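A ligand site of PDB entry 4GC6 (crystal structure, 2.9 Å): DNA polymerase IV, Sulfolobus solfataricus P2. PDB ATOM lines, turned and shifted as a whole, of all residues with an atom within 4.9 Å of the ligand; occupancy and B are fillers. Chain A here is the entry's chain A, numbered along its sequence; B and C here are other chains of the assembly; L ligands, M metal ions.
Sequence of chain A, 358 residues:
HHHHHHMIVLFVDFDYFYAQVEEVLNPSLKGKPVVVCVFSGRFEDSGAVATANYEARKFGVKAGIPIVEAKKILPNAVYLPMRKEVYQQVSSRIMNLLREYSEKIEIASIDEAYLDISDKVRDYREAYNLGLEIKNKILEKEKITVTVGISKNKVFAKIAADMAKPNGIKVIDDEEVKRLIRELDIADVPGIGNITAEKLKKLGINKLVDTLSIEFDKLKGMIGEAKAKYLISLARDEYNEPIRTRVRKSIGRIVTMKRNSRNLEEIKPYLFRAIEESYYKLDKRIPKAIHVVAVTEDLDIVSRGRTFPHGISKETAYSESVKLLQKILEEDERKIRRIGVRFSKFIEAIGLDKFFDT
O of Asp 111 sits at hydrogen-bond distance from N of Phe 14 of chain A (3.1 Å).
N1 of DG 5 of chain B sits close to a nitrogen (N4) of the ligand (3.4 Å).
Ala 50 touches the ligand (O to C10, 3.5 Å).
CB of Ala 63 touches N5 of the ligand, at 3.96 Å.
CG2 of Ile 110 touches C4 of the ligand, at 3.8 Å.
Asp 111 touches the ligand.
Hydrophobic or aromatic side chains that line the ligand: Phe 17, Tyr 18, Ala 63 and Ile 110.
Along chain A the residues within 4 Å of the ligand span positions 16 to 111.
O1 of the ligand lies within salt-bridge range of NH1 of Arg 57 (2.9 Å).
O3 of the ligand lies within hydrogen-bond range of N of Phe 17, 2.9 Å away.
O4 of DT 4 of chain B lies within hydrogen-bond range of a nitrogen (N5) of the ligand (3.2 Å).
An oxygen (O3) of the ligand lies close to the backbone NH of Tyr 16 (3.4 Å).
N of Tyr 18 sits at hydrogen-bond distance from O5 of the ligand (3.1 Å).
The side-chain hydroxyl (OG1) of Thr 51 lies close to an oxygen (O5) of the ligand.
N4 of DC 14 of chain C sits at hydrogen-bond distance from a nitrogen (N5) of the ligand (3.3 Å).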
ATOM      1  N   ASP A  13     -17.811 -15.223   1.404  1.00  0.00           N
ATOM      2  CA  ASP A  13     -18.066 -15.010  -0.020  1.00  0.00           C
ATOM      3  C   ASP A  13     -16.783 -15.289  -0.808  1.00  0.00           C
ATOM      4  O   ASP A  13     -15.796 -14.558  -0.673  1.00  0.00           O
ATOM      5  CB  ASP A  13     -18.543 -13.559  -0.210  1.00  0.00           C
ATOM      6  CG  ASP A  13     -18.719 -13.155  -1.663  1.00  0.00           C
ATOM      7  OD1 ASP A  13     -17.731 -12.694  -2.292  1.00  0.00           O
ATOM      8  OD2 ASP A  13     -19.850 -13.237  -2.183  1.00  0.00           O
ATOM      9  N   PHE A  14     -16.794 -16.353  -1.624  1.00  0.00           N
ATOM     10  CA  PHE A  14     -15.574 -16.830  -2.282  1.00  0.00           C
ATOM     11  C   PHE A  14     -15.169 -15.937  -3.452  1.00  0.00           C
ATOM     12  O   PHE A  14     -15.817 -15.985  -4.483  1.00  0.00           O
ATOM     13  CB  PHE A  14     -15.732 -18.241  -2.872  1.00  0.00           C
ATOM     14  CG  PHE A  14     -16.209 -19.280  -1.902  1.00  0.00           C
ATOM     15  CD1 PHE A  14     -16.260 -19.030  -0.526  1.00  0.00           C
ATOM     16  CD2 PHE A  14     -16.617 -20.516  -2.356  1.00  0.00           C
ATOM     17  CE1 PHE A  14     -16.715 -19.997   0.364  1.00  0.00           C
ATOM     18  CE2 PHE A  14     -17.071 -21.499  -1.475  1.00  0.00           C
ATOM     19  CZ  PHE A  14     -17.109 -21.233  -0.101  1.00  0.00           C
ATOM     20  N   ASP A  15     -14.076 -15.202  -3.314  1.00  0.00           N
ATOM     21  CA  ASP A  15     -13.624 -14.245  -4.344  1.00  0.00           C
ATOM     22  C   ASP A  15     -13.627 -14.740  -5.806  1.00  0.00           C
ATOM     23  O   ASP A  15     -13.190 -15.863  -6.069  1.00  0.00           O
ATOM     24  CB  ASP A  15     -12.238 -13.680  -3.972  1.00  0.00           C
ATOM     25  CG  ASP A  15     -12.250 -12.925  -2.662  1.00  0.00           C
ATOM     26  OD1 ASP A  15     -13.253 -12.229  -2.409  1.00  0.00           O
ATOM     27  OD2 ASP A  15     -11.272 -13.035  -1.876  1.00  0.00           O
ATOM     28  N   TYR A  16     -14.139 -13.885  -6.708  1.00  0.00           N
ATOM     29  CA  TYR A  16     -14.233 -14.110  -8.168  1.00  0.00           C
ATOM     30  C   TYR A  16     -14.295 -15.588  -8.615  1.00  0.00           C
ATOM     31  O   TYR A  16     -13.574 -16.038  -9.506  1.00  0.00           O
ATOM     32  CB  TYR A  16     -13.169 -13.293  -8.938  1.00  0.00           C
ATOM     33  CG  TYR A  16     -11.722 -13.623  -8.620  1.00  0.00           C
ATOM     34  CD1 TYR A  16     -10.954 -14.396  -9.494  1.00  0.00           C
ATOM     35  CD2 TYR A  16     -11.128 -13.143  -7.458  1.00  0.00           C
ATOM     36  CE1 TYR A  16      -9.632 -14.708  -9.210  1.00  0.00           C
ATOM     37  CE2 TYR A  16      -9.806 -13.454  -7.164  1.00  0.00           C
ATOM     38  CZ  TYR A  16      -9.058 -14.237  -8.046  1.00  0.00           C
ATOM     39  OH  TYR A  16      -7.744 -14.541  -7.752  1.00  0.00           O
ATOM     40  N   PHE A  17     -15.241 -16.283  -8.009  1.00  0.00           N
ATOM     41  CA  PHE A  17     -15.207 -17.726  -7.831  1.00  0.00           C
ATOM     42  C   PHE A  17     -14.831 -18.662  -9.001  1.00  0.00           C
ATOM     43  O   PHE A  17     -13.891 -19.435  -8.876  1.00  0.00           O
ATOM     44  CB  PHE A  17     -16.475 -18.196  -7.141  1.00  0.00           C
ATOM     45  CG  PHE A  17     -16.449 -19.641  -6.790  1.00  0.00           C
ATOM     46  CD1 PHE A  17     -15.452 -20.139  -5.976  1.00  0.00           C
ATOM     47  CD2 PHE A  17     -17.416 -20.504  -7.283  1.00  0.00           C
ATOM     48  CE1 PHE A  17     -15.423 -21.487  -5.647  1.00  0.00           C
ATOM     49  CE2 PHE A  17     -17.382 -21.830  -6.957  1.00  0.00           C
ATOM     50  CZ  PHE A  17     -16.378 -22.320  -6.135  1.00  0.00           C
ATOM     51  N   TYR A  18     -15.556 -18.634 -10.107  1.00  0.00           N
ATOM     52  CA  TYR A  18     -15.247 -19.599 -11.159  1.00  0.00           C
ATOM     53  C   TYR A  18     -13.875 -19.315 -11.751  1.00  0.00           C
ATOM     54  O   TYR A  18     -13.102 -20.232 -12.032  1.00  0.00           O
ATOM     55  CB  TYR A  18     -16.259 -19.578 -12.305  1.00  0.00           C
ATOM     56  CG  TYR A  18     -17.627 -20.107 -11.965  1.00  0.00           C
ATOM     57  CD1 TYR A  18     -17.932 -20.540 -10.688  1.00  0.00           C
ATOM     58  CD2 TYR A  18     -18.620 -20.148 -12.934  1.00  0.00           C
ATOM     59  CE1 TYR A  18     -19.179 -21.015 -10.373  1.00  0.00           C
ATOM     60  CE2 TYR A  18     -19.874 -20.634 -12.637  1.00  0.00           C
ATOM     61  CZ  TYR A  18     -20.152 -21.049 -11.354  1.00  0.00           C
ATOM     62  OH  TYR A  18     -21.408 -21.520 -11.049  1.00  0.00           O
ATOM     63  N   VAL A  49     -20.850 -14.029 -20.571  1.00  0.00           N
ATOM     64  CA  VAL A  49     -19.791 -14.223 -19.598  1.00  0.00           C
ATOM     65  C   VAL A  49     -20.353 -14.667 -18.242  1.00  0.00           C
ATOM     66  O   VAL A  49     -21.317 -14.088 -17.735  1.00  0.00           O
ATOM     67  CB  VAL A  49     -18.910 -12.943 -19.495  1.00  0.00           C
ATOM     68  CG1 VAL A  49     -18.122 -12.884 -18.201  1.00  0.00           C
ATOM     69  CG2 VAL A  49     -17.991 -12.892 -20.684  1.00  0.00           C
ATOM     70  N   ALA A  50     -19.764 -15.711 -17.666  1.00  0.00           N
ATOM     71  CA  ALA A  50     -20.226 -16.193 -16.362  1.00  0.00           C
ATOM     72  C   ALA A  50     -19.642 -15.346 -15.235  1.00  0.00           C
ATOM     73  O   ALA A  50     -20.368 -14.824 -14.403  1.00  0.00           O
ATOM     74  CB  ALA A  50     -19.859 -17.669 -16.161  1.00  0.00           C
ATOM     75  N   THR A  51     -18.325 -15.230 -15.207  1.00  0.00           N
ATOM     76  CA  THR A  51     -17.643 -14.365 -14.260  1.00  0.00           C
ATOM     77  C   THR A  51     -16.295 -14.079 -14.882  1.00  0.00           C
ATOM     78  O   THR A  51     -15.974 -14.649 -15.933  1.00  0.00           O
ATOM     79  CB  THR A  51     -17.507 -15.043 -12.851  1.00  0.00           C
ATOM     80  OG1 THR A  51     -17.367 -14.048 -11.834  1.00  0.00           O
ATOM     81  CG2 THR A  51     -16.339 -16.030 -12.806  1.00  0.00           C
ATOM     82  N   ARG A  57     -11.988  -7.576 -14.765  1.00  0.00           N
ATOM     83  CA  ARG A  57     -13.181  -6.883 -14.307  1.00  0.00           C
ATOM     84  C   ARG A  57     -12.942  -5.395 -14.227  1.00  0.00           C
ATOM     85  O   ARG A  57     -13.877  -4.598 -14.335  1.00  0.00           O
ATOM     86  CB  ARG A  57     -13.670  -7.428 -12.963  1.00  0.00           C
ATOM     87  CG  ARG A  57     -15.157  -7.171 -12.714  1.00  0.00           C
ATOM     88  CD  ARG A  57     -15.659  -7.863 -11.452  1.00  0.00           C
ATOM     89  NE  ARG A  57     -15.325  -9.292 -11.426  1.00  0.00           N
ATOM     90  CZ  ARG A  57     -15.695 -10.119 -10.449  1.00  0.00           C
ATOM     91  NH1 ARG A  57     -16.425  -9.690  -9.434  1.00  0.00           N
ATOM     92  NH2 ARG A  57     -15.339 -11.397 -10.505  1.00  0.00           N
ATOM     93  N   ALA A  63     -19.911 -10.201 -15.266  1.00  0.00           N
ATOM     94  CA  ALA A  63     -20.869 -11.267 -15.543  1.00  0.00           C
ATOM     95  C   ALA A  63     -22.087 -10.703 -16.269  1.00  0.00           C
ATOM     96  O   ALA A  63     -22.632  -9.675 -15.866  1.00  0.00           O
ATOM     97  CB  ALA A  63     -21.277 -11.952 -14.248  1.00  0.00           C
ATOM     98  N   GLY A  64     -22.500 -11.354 -17.341  1.00  0.00           N
ATOM     99  CA  GLY A  64     -23.713 -10.940 -18.019  1.00  0.00           C
ATOM    100  C   GLY A  64     -23.551 -10.273 -19.366  1.00  0.00           C
ATOM    101  O   GLY A  64     -24.485 -10.252 -20.154  1.00  0.00           O
ATOM    102  N   ILE A 110     -23.569 -21.524  -4.529  1.00  0.00           N
ATOM    103  CA  ILE A 110     -22.303 -22.213  -4.781  1.00  0.00           C
ATOM    104  C   ILE A 110     -21.054 -21.522  -4.184  1.00  0.00           C
ATOM    105  O   ILE A 110     -20.016 -22.172  -4.020  1.00  0.00           O
ATOM    106  CB  ILE A 110     -22.067 -22.431  -6.294  1.00  0.00           C
ATOM    107  CG1 ILE A 110     -21.176 -23.645  -6.525  1.00  0.00           C
ATOM    108  CG2 ILE A 110     -21.473 -21.172  -6.957  1.00  0.00           C
ATOM    109  CD1 ILE A 110     -21.138 -24.087  -7.937  1.00  0.00           C
ATOM    110  N   ASP A 111     -21.110 -20.227  -3.837  1.00  0.00           N
ATOM    111  CA  ASP A 111     -19.950 -19.581  -3.239  1.00  0.00           C
ATOM    112  C   ASP A 111     -20.257 -18.671  -2.049  1.00  0.00           C
ATOM    113  O   ASP A 111     -19.566 -17.665  -1.798  1.00  0.00           O
ATOM    114  CB  ASP A 111     -19.139 -18.801  -4.280  1.00  0.00           C
ATOM    115  CG  ASP A 111     -19.852 -17.525  -4.776  1.00  0.00           C
ATOM    116  OD1 ASP A 111     -20.920 -17.105  -4.252  1.00  0.00           O
ATOM    117  OD2 ASP A 111     -19.286 -16.915  -5.698  1.00  0.00           O
ATOM    118  N   LYS A 165     -14.666  -6.936  -0.514  1.00  0.00           N
ATOM    119  CA  LYS A 165     -14.259  -7.691  -1.699  1.00  0.00           C
ATOM    120  C   LYS A 165     -13.134  -7.004  -2.477  1.00  0.00           C
ATOM    121  O   LYS A 165     -13.168  -5.783  -2.658  1.00  0.00           O
ATOM    122  CB  LYS A 165     -15.433  -7.846  -2.671  1.00  0.00           C
ATOM    123  CG  LYS A 165     -16.522  -8.791  -2.288  1.00  0.00           C
ATOM    124  CD  LYS A 165     -17.614  -8.753  -3.340  1.00  0.00           C
ATOM    125  CE  LYS A 165     -18.727  -9.746  -3.040  1.00  0.00           C
ATOM    126  NZ  LYS A 165     -19.959  -9.457  -3.841  1.00  0.00           N
ATOM    127  P    DT B   4     -27.745 -15.708 -24.473  1.00  0.00           P
ATOM    128  OP1  DT B   4     -27.983 -16.483 -25.723  1.00  0.00           O
ATOM    129  OP2  DT B   4     -28.888 -15.101 -23.755  1.00  0.00           O
ATOM    130  O5'  DT B   4     -26.968 -16.610 -23.422  1.00  0.00           O
ATOM    131  C5'  DT B   4     -25.894 -17.415 -23.807  1.00  0.00           C
ATOM    132  C4'  DT B   4     -25.714 -18.465 -22.738  1.00  0.00           C
ATOM    133  O4'  DT B   4     -25.313 -17.885 -21.464  1.00  0.00           O
ATOM    134  C3'  DT B   4     -26.946 -19.286 -22.391  1.00  0.00           C
ATOM    135  O3'  DT B   4     -26.427 -20.551 -21.994  1.00  0.00           O
ATOM    136  C2'  DT B   4     -27.557 -18.497 -21.226  1.00  0.00           C
ATOM    137  C1'  DT B   4     -26.282 -18.164 -20.465  1.00  0.00           C
ATOM    138  N1   DT B   4     -26.266 -16.964 -19.596  1.00  0.00           N
ATOM    139  C2   DT B   4     -25.620 -17.036 -18.368  1.00  0.00           C
ATOM    140  O2   DT B   4     -25.083 -18.039 -17.955  1.00  0.00           O
ATOM    141  N3   DT B   4     -25.625 -15.867 -17.626  1.00  0.00           N
ATOM    142  C4   DT B   4     -26.192 -14.661 -17.991  1.00  0.00           C
ATOM    143  O4   DT B   4     -26.151 -13.674 -17.249  1.00  0.00           O
ATOM    144  C5   DT B   4     -26.845 -14.663 -19.301  1.00  0.00           C
ATOM    145  C7   DT B   4     -27.513 -13.430 -19.835  1.00  0.00           C
ATOM    146  C6   DT B   4     -26.850 -15.796 -20.037  1.00  0.00           C
ATOM    147  P    DG B   5     -27.347 -21.864 -22.091  1.00  0.00           P
ATOM    148  OP1  DG B   5     -27.090 -22.508 -23.411  1.00  0.00           O
ATOM    149  OP2  DG B   5     -28.717 -21.472 -21.714  1.00  0.00           O
ATOM    150  O5'  DG B   5     -26.819 -22.798 -20.898  1.00  0.00           O
ATOM    151  C5'  DG B   5     -25.978 -22.319 -19.853  1.00  0.00           C
ATOM    152  C4'  DG B   5     -26.622 -22.261 -18.474  1.00  0.00           C
ATOM    153  O4'  DG B   5     -26.694 -20.900 -17.983  1.00  0.00           O
ATOM    154  C3'  DG B   5     -28.038 -22.792 -18.292  1.00  0.00           C
ATOM    155  O3'  DG B   5     -28.046 -23.430 -17.019  1.00  0.00           O
ATOM    156  C2'  DG B   5     -28.862 -21.517 -18.214  1.00  0.00           C
ATOM    157  C1'  DG B   5     -27.907 -20.777 -17.301  1.00  0.00           C
ATOM    158  N9   DG B   5     -28.220 -19.377 -17.102  1.00  0.00           N
ATOM    159  C8   DG B   5     -28.918 -18.510 -17.921  1.00  0.00           C
ATOM    160  N7   DG B   5     -29.029 -17.322 -17.406  1.00  0.00           N
ATOM    161  C5   DG B   5     -28.360 -17.398 -16.169  1.00  0.00           C
ATOM    162  C6   DG B   5     -28.146 -16.423 -15.144  1.00  0.00           C
ATOM    163  O6   DG B   5     -28.517 -15.230 -15.127  1.00  0.00           O
ATOM    164  N1   DG B   5     -27.424 -16.948 -14.056  1.00  0.00           N
ATOM    165  C2   DG B   5     -26.977 -18.252 -13.983  1.00  0.00           C
ATOM    166  N2   DG B   5     -26.309 -18.572 -12.877  1.00  0.00           N
ATOM    167  N3   DG B   5     -27.168 -19.179 -14.925  1.00  0.00           N
ATOM    168  C4   DG B   5     -27.857 -18.676 -15.982  1.00  0.00           C
ATOM    169  P    DC C  14     -25.412 -11.840  -4.893  1.00  0.00           P
ATOM    170  OP1  DC C  14     -24.721 -11.728  -3.600  1.00  0.00           O
ATOM    171  OP2  DC C  14     -25.306 -10.719  -5.869  1.00  0.00           O
ATOM    172  O5'  DC C  14     -24.955 -13.211  -5.580  1.00  0.00           O
ATOM    173  C5'  DC C  14     -25.339 -14.419  -4.908  1.00  0.00           C
ATOM    174  C4'  DC C  14     -24.950 -15.640  -5.720  1.00  0.00           C
ATOM    175  O4'  DC C  14     -25.754 -15.682  -6.923  1.00  0.00           O
ATOM    176  C3'  DC C  14     -23.503 -15.671  -6.197  1.00  0.00           C
ATOM    177  O3'  DC C  14     -23.021 -17.030  -6.201  1.00  0.00           O
ATOM    178  C2'  DC C  14     -23.616 -15.076  -7.608  1.00  0.00           C
ATOM    179  C1'  DC C  14     -24.884 -15.801  -8.048  1.00  0.00           C
ATOM    180  N1   DC C  14     -25.634 -15.333  -9.288  1.00  0.00           N
ATOM    181  C2   DC C  14     -25.946 -16.300 -10.277  1.00  0.00           C
ATOM    182  O2   DC C  14     -25.567 -17.477 -10.094  1.00  0.00           O
ATOM    183  N3   DC C  14     -26.629 -15.920 -11.410  1.00  0.00           N
ATOM    184  C4   DC C  14     -27.014 -14.637 -11.535  1.00  0.00           C
ATOM    185  N4   DC C  14     -27.676 -14.310 -12.653  1.00  0.00           N
ATOM    186  C5   DC C  14     -26.712 -13.635 -10.540  1.00  0.00           C
ATOM    187  C6   DC C  14     -26.031 -14.020  -9.446  1.00  0.00           C
HETATM  188  O1  LIG L   1     -17.935 -12.089  -9.041  1.00  0.00           O
HETATM  189  P1  LIG L   1     -18.446 -13.269  -8.142  1.00  0.00           P
HETATM  190  O2  LIG L   1     -19.068 -12.726  -6.865  1.00  0.00           O
HETATM  191  O3  LIG L   1     -17.291 -14.218  -7.949  1.00  0.00           O
HETATM  192  O4  LIG L   1     -19.593 -14.061  -8.834  1.00  0.00           O
HETATM  193  C1  LIG L   1     -20.057 -15.225  -8.212  1.00  0.00           C
HETATM  194  C2  LIG L   1     -20.091 -16.493  -9.031  1.00  0.00           C
HETATM  195  C3  LIG L   1     -21.481 -17.071  -9.208  1.00  0.00           C
HETATM  196  C4  LIG L   1     -20.473 -17.774  -8.319  1.00  0.00           C
HETATM  197  C5  LIG L   1     -19.429 -16.559 -10.370  1.00  0.00           C
HETATM  198  O5  LIG L   1     -18.156 -17.000 -10.228  1.00  0.00           O
HETATM  199  C6  LIG L   1     -20.258 -17.489 -11.187  1.00  0.00           C
HETATM  200  C7  LIG L   1     -21.644 -17.350 -10.697  1.00  0.00           C
HETATM  201  N1  LIG L   1     -22.379 -16.268 -11.359  1.00  0.00           N
HETATM  202  C8  LIG L   1     -22.567 -15.033 -10.855  1.00  0.00           C
HETATM  203  N2  LIG L   1     -23.277 -14.311 -11.736  1.00  0.00           N
HETATM  204  C9  LIG L   1     -23.584 -15.053 -12.825  1.00  0.00           C
HETATM  205  C10 LIG L   1     -23.007 -16.316 -12.584  1.00  0.00           C
HETATM  206  N3  LIG L   1     -23.135 -17.291 -13.513  1.00  0.00           N
HETATM  207  C11 LIG L   1     -23.811 -17.062 -14.658  1.00  0.00           C
HETATM  208  N4  LIG L   1     -24.368 -15.870 -14.912  1.00  0.00           N
HETATM  209  C12 LIG L   1     -24.278 -14.849 -14.046  1.00  0.00           C
HETATM  210  N5  LIG L   1     -24.889 -13.583 -14.356  1.00  0.00           N
HETATM  211 CA    CA M   1     -18.004 -14.453  -4.750  1.00  0.00          CA
HETATM  212 CA    CA M   2     -21.516 -12.885  -4.600  1.00  0.00          CA
